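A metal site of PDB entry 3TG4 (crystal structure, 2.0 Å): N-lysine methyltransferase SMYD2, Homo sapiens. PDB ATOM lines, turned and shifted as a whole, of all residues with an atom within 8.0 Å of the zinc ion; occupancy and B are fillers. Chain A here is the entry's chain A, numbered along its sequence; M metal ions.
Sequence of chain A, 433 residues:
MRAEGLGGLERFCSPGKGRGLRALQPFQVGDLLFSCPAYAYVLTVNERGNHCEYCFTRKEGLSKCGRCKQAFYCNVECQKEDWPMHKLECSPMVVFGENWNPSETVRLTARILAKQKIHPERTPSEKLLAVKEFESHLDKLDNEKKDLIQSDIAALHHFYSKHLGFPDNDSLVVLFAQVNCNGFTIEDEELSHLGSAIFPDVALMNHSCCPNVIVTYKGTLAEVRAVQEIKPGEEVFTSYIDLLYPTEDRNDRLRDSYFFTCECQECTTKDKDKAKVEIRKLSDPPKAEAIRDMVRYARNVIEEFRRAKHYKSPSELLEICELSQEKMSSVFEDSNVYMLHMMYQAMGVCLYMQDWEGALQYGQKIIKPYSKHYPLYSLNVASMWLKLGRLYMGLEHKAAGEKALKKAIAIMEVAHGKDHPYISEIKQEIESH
The side-chain sulfur of Cys 52 sits close to the backbone NH of Tyr 54. The side-chain sulfur (SG) of Cys 55 sits close to the side-chain hydroxyl (OG1) of Thr 57 (3.2 Å). The backbone carbonyl oxygen (O) of Cys 74 sits at hydrogen-bond distance from the side-chain amino group (NZ) of Lys 59, 2.6 Å away. The backbone NH (N) of Cys 52 is in hydrogen-bond range of the backbone carbonyl oxygen (O) of Thr 57. The side-chain amide oxygen (OD1) of Asn 75 lies within hydrogen-bond range of the backbone NH (N) of Cys 78, at 2.9 Å.
Four residues have an atom within 4 Å of the zinc ion: Cys 52, Cys 55, Cys 74 and Cys 78.
The zinc ion is bound by the side-chain sulfur (SG) of Cys 55, 2.3 Å away. The side-chain sulfur (SG) of Cys 78 is bound to the zinc ion (2.3 Å). The side-chain sulfur (SG) of Cys 52 is bound to the zinc ion (2.3 Å). The zinc ion is bound by SG of Cys 74.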
ATOM      1  N   HIS A  51      10.086  14.627  15.425  1.00  0.00           N
ATOM      2  CA  HIS A  51      10.759  13.715  16.339  1.00  0.00           C
ATOM      3  C   HIS A  51      11.020  12.379  15.652  1.00  0.00           C
ATOM      4  O   HIS A  51      10.220  11.938  14.809  1.00  0.00           O
ATOM      5  CB  HIS A  51       9.908  13.437  17.575  1.00  0.00           C
ATOM      6  CG  HIS A  51       9.743  14.615  18.478  1.00  0.00           C
ATOM      7  ND1 HIS A  51      10.386  14.718  19.695  1.00  0.00           N
ATOM      8  CD2 HIS A  51       9.025  15.757  18.331  1.00  0.00           C
ATOM      9  CE1 HIS A  51      10.070  15.869  20.255  1.00  0.00           C
ATOM     10  NE2 HIS A  51       9.247  16.519  19.450  1.00  0.00           N
ATOM     11  N   CYS A  52      12.131  11.738  16.014  1.00  0.00           N
ATOM     12  CA  CYS A  52      12.428  10.375  15.577  1.00  0.00           C
ATOM     13  C   CYS A  52      11.341   9.405  16.048  1.00  0.00           C
ATOM     14  O   CYS A  52      10.960   9.440  17.226  1.00  0.00           O
ATOM     15  CB  CYS A  52      13.762   9.947  16.154  1.00  0.00           C
ATOM     16  SG  CYS A  52      14.340   8.303  15.691  1.00  0.00           S
ATOM     17  N   GLU A  53      10.883   8.516  15.149  1.00  0.00           N
ATOM     18  CA  GLU A  53       9.826   7.537  15.466  1.00  0.00           C
ATOM     19  C   GLU A  53      10.359   6.596  16.509  1.00  0.00           C
ATOM     20  O   GLU A  53       9.617   6.131  17.372  1.00  0.00           O
ATOM     21  CB  GLU A  53       9.445   6.688  14.231  1.00  0.00           C
ATOM     22  CG  GLU A  53       9.013   7.454  13.014  1.00  0.00           C
ATOM     23  CD  GLU A  53       7.529   7.795  12.997  1.00  0.00           C
ATOM     24  OE1 GLU A  53       6.734   7.022  13.553  1.00  0.00           O
ATOM     25  OE2 GLU A  53       7.168   8.816  12.383  1.00  0.00           O
ATOM     26  N   TYR A  54      11.649   6.300  16.415  1.00  0.00           N
ATOM     27  CA  TYR A  54      12.228   5.261  17.246  1.00  0.00           C
ATOM     28  C   TYR A  54      12.554   5.708  18.675  1.00  0.00           C
ATOM     29  O   TYR A  54      12.174   5.033  19.623  1.00  0.00           O
ATOM     30  CB  TYR A  54      13.466   4.627  16.589  1.00  0.00           C
ATOM     31  CG  TYR A  54      14.006   3.492  17.417  1.00  0.00           C
ATOM     32  CD1 TYR A  54      15.219   3.599  18.106  1.00  0.00           C
ATOM     33  CD2 TYR A  54      13.267   2.311  17.560  1.00  0.00           C
ATOM     34  CE1 TYR A  54      15.678   2.567  18.907  1.00  0.00           C
ATOM     35  CE2 TYR A  54      13.725   1.268  18.354  1.00  0.00           C
ATOM     36  CZ  TYR A  54      14.927   1.407  19.029  1.00  0.00           C
ATOM     37  OH  TYR A  54      15.368   0.374  19.808  1.00  0.00           O
ATOM     38  N   CYS A  55      13.304   6.800  18.820  1.00  0.00           N
ATOM     39  CA  CYS A  55      13.803   7.237  20.126  1.00  0.00           C
ATOM     40  C   CYS A  55      13.186   8.557  20.612  1.00  0.00           C
ATOM     41  O   CYS A  55      13.491   9.027  21.716  1.00  0.00           O
ATOM     42  CB  CYS A  55      15.333   7.340  20.072  1.00  0.00           C
ATOM     43  SG  CYS A  55      15.917   8.753  19.128  1.00  0.00           S
ATOM     44  N   PHE A  56      12.326   9.163  19.788  1.00  0.00           N
ATOM     45  CA  PHE A  56      11.599  10.403  20.153  1.00  0.00           C
ATOM     46  C   PHE A  56      12.471  11.667  20.260  1.00  0.00           C
ATOM     47  O   PHE A  56      11.978  12.726  20.646  1.00  0.00           O
ATOM     48  CB  PHE A  56      10.768  10.206  21.447  1.00  0.00           C
ATOM     49  CG  PHE A  56       9.434   9.499  21.225  1.00  0.00           C
ATOM     50  CD1 PHE A  56       9.260   8.549  20.207  1.00  0.00           C
ATOM     51  CD2 PHE A  56       8.356   9.762  22.087  1.00  0.00           C
ATOM     52  CE1 PHE A  56       8.024   7.885  20.028  1.00  0.00           C
ATOM     53  CE2 PHE A  56       7.130   9.111  21.926  1.00  0.00           C
ATOM     54  CZ  PHE A  56       6.960   8.166  20.887  1.00  0.00           C
ATOM     55  N   THR A  57      13.748  11.583  19.893  1.00  0.00           N
ATOM     56  CA  THR A  57      14.637  12.752  19.868  1.00  0.00           C
ATOM     57  C   THR A  57      14.139  13.816  18.892  1.00  0.00           C
ATOM     58  O   THR A  57      13.810  13.520  17.733  1.00  0.00           O
ATOM     59  CB  THR A  57      16.069  12.328  19.477  1.00  0.00           C
ATOM     60  OG1 THR A  57      16.627  11.565  20.552  1.00  0.00           O
ATOM     61  CG2 THR A  57      16.972  13.556  19.212  1.00  0.00           C
ATOM     62  N   ARG A  58      14.096  15.068  19.353  1.00  0.00           N
ATOM     63  CA  ARG A  58      13.751  16.212  18.491  1.00  0.00           C
ATOM     64  C   ARG A  58      14.984  16.672  17.728  1.00  0.00           C
ATOM     65  O   ARG A  58      16.021  16.953  18.320  1.00  0.00           O
ATOM     66  CB  ARG A  58      13.152  17.374  19.294  1.00  0.00           C
ATOM     67  CG  ARG A  58      12.718  18.558  18.427  1.00  0.00           C
ATOM     68  CD  ARG A  58      11.625  19.408  19.067  1.00  0.00           C
ATOM     69  NE  ARG A  58      12.077  20.131  20.259  1.00  0.00           N
ATOM     70  CZ  ARG A  58      12.816  21.241  20.263  1.00  0.00           C
ATOM     71  NH1 ARG A  58      13.235  21.785  19.132  1.00  0.00           N
ATOM     72  NH2 ARG A  58      13.152  21.815  21.411  1.00  0.00           N
ATOM     73  N   LYS A  59      14.852  16.776  16.405  1.00  0.00           N
ATOM     74  CA  LYS A  59      15.959  17.176  15.560  1.00  0.00           C
ATOM     75  C   LYS A  59      15.419  17.703  14.231  1.00  0.00           C
ATOM     76  O   LYS A  59      14.430  17.176  13.729  1.00  0.00           O
ATOM     77  CB  LYS A  59      16.910  15.973  15.374  1.00  0.00           C
ATOM     78  CG  LYS A  59      17.687  15.920  14.117  1.00  0.00           C
ATOM     79  CD  LYS A  59      18.586  14.716  14.131  1.00  0.00           C
ATOM     80  CE  LYS A  59      18.954  14.305  12.739  1.00  0.00           C
ATOM     81  NZ  LYS A  59      19.988  13.247  12.744  1.00  0.00           N
ATOM     82  N   LEU A  62      15.476  15.225  10.102  1.00  0.00           N
ATOM     83  CA  LEU A  62      15.372  13.791  10.319  1.00  0.00           C
ATOM     84  C   LEU A  62      15.357  13.060   8.988  1.00  0.00           C
ATOM     85  O   LEU A  62      14.817  13.581   8.000  1.00  0.00           O
ATOM     86  CB  LEU A  62      14.076  13.490  11.097  1.00  0.00           C
ATOM     87  CG  LEU A  62      14.096  13.882  12.566  1.00  0.00           C
ATOM     88  CD1 LEU A  62      12.657  13.970  13.121  1.00  0.00           C
ATOM     89  CD2 LEU A  62      14.939  12.884  13.358  1.00  0.00           C
ATOM     90  N   PHE A  72      10.155   9.264  10.122  1.00  0.00           N
ATOM     91  CA  PHE A  72      11.459   9.963  10.167  1.00  0.00           C
ATOM     92  C   PHE A  72      12.334   9.521  11.337  1.00  0.00           C
ATOM     93  O   PHE A  72      11.832   9.201  12.418  1.00  0.00           O
ATOM     94  CB  PHE A  72      11.245  11.490  10.211  1.00  0.00           C
ATOM     95  CG  PHE A  72      10.483  12.042   9.026  1.00  0.00           C
ATOM     96  CD1 PHE A  72      11.140  12.707   8.016  1.00  0.00           C
ATOM     97  CD2 PHE A  72       9.096  11.892   8.939  1.00  0.00           C
ATOM     98  CE1 PHE A  72      10.441  13.241   6.937  1.00  0.00           C
ATOM     99  CE2 PHE A  72       8.383  12.413   7.856  1.00  0.00           C
ATOM    100  CZ  PHE A  72       9.061  13.085   6.846  1.00  0.00           C
ATOM    101  N   TYR A  73      13.641   9.489  11.115  1.00  0.00           N
ATOM    102  CA  TYR A  73      14.592   8.891  12.057  1.00  0.00           C
ATOM    103  C   TYR A  73      15.857   9.722  12.202  1.00  0.00           C
ATOM    104  O   TYR A  73      16.199  10.498  11.311  1.00  0.00           O
ATOM    105  CB  TYR A  73      14.979   7.484  11.587  1.00  0.00           C
ATOM    106  CG  TYR A  73      13.801   6.560  11.464  1.00  0.00           C
ATOM    107  CD1 TYR A  73      13.277   5.905  12.583  1.00  0.00           C
ATOM    108  CD2 TYR A  73      13.196   6.342  10.229  1.00  0.00           C
ATOM    109  CE1 TYR A  73      12.197   5.057  12.463  1.00  0.00           C
ATOM    110  CE2 TYR A  73      12.102   5.493  10.111  1.00  0.00           C
ATOM    111  CZ  TYR A  73      11.620   4.840  11.223  1.00  0.00           C
ATOM    112  OH  TYR A  73      10.553   4.010  11.099  1.00  0.00           O
ATOM    113  N   CYS A  74      16.546   9.573  13.326  1.00  0.00           N
ATOM    114  CA  CYS A  74      17.820  10.262  13.572  1.00  0.00           C
ATOM    115  C   CYS A  74      18.882   9.876  12.543  1.00  0.00           C
ATOM    116  O   CYS A  74      19.689  10.711  12.117  1.00  0.00           O
ATOM    117  CB  CYS A  74      18.370   9.878  14.951  1.00  0.00           C
ATOM    118  SG  CYS A  74      17.387  10.351  16.337  1.00  0.00           S
ATOM    119  N   ASN A  75      18.874   8.608  12.154  1.00  0.00           N
ATOM    120  CA  ASN A  75      19.973   8.010  11.368  1.00  0.00           C
ATOM    121  C   ASN A  75      19.524   6.608  10.927  1.00  0.00           C
ATOM    122  O   ASN A  75      18.398   6.211  11.244  1.00  0.00           O
ATOM    123  CB  ASN A  75      21.261   7.945  12.199  1.00  0.00           C
ATOM    124  CG  ASN A  75      21.120   7.103  13.485  1.00  0.00           C
ATOM    125  OD1 ASN A  75      20.100   6.440  13.725  1.00  0.00           O
ATOM    126  ND2 ASN A  75      22.177   7.122  14.293  1.00  0.00           N
ATOM    127  N   GLU A  77      20.479   3.713  12.016  1.00  0.00           N
ATOM    128  CA  GLU A  77      20.357   2.854  13.204  1.00  0.00           C
ATOM    129  C   GLU A  77      18.952   2.898  13.774  1.00  0.00           C
ATOM    130  O   GLU A  77      18.334   1.863  13.992  1.00  0.00           O
ATOM    131  CB  GLU A  77      21.365   3.248  14.286  1.00  0.00           C
ATOM    132  CG  GLU A  77      22.833   3.030  13.907  1.00  0.00           C
ATOM    133  CD  GLU A  77      23.791   3.731  14.865  1.00  0.00           C
ATOM    134  OE1 GLU A  77      23.341   4.561  15.685  1.00  0.00           O
ATOM    135  OE2 GLU A  77      24.999   3.455  14.799  1.00  0.00           O
ATOM    136  N   CYS A  78      18.457   4.104  14.024  1.00  0.00           N
ATOM    137  CA  CYS A  78      17.099   4.306  14.490  1.00  0.00           C
ATOM    138  C   CYS A  78      16.087   3.753  13.467  1.00  0.00           C
ATOM    139  O   CYS A  78      15.106   3.114  13.857  1.00  0.00           O
ATOM    140  CB  CYS A  78      16.854   5.783  14.760  1.00  0.00           C
ATOM    141  SG  CYS A  78      17.476   6.346  16.355  1.00  0.00           S
ATOM    142  N   GLN A  79      16.322   3.986  12.184  1.00  0.00           N
ATOM    143  CA  GLN A  79      15.435   3.451  11.146  1.00  0.00           C
ATOM    144  C   GLN A  79      15.364   1.905  11.147  1.00  0.00           C
ATOM    145  O   GLN A  79      14.269   1.313  11.054  1.00  0.00           O
ATOM    146  CB  GLN A  79      15.810   3.974   9.750  1.00  0.00           C
ATOM    147  CG  GLN A  79      14.854   3.478   8.655  1.00  0.00           C
ATOM    148  CD  GLN A  79      15.166   4.021   7.272  1.00  0.00           C
ATOM    149  OE1 GLN A  79      14.424   3.761   6.313  1.00  0.00           O
ATOM    150  NE2 GLN A  79      16.260   4.743   7.148  1.00  0.00           N
HETATM  151 ZN    ZN M   1      16.350   8.306  16.893  1.00  0.00          ZN
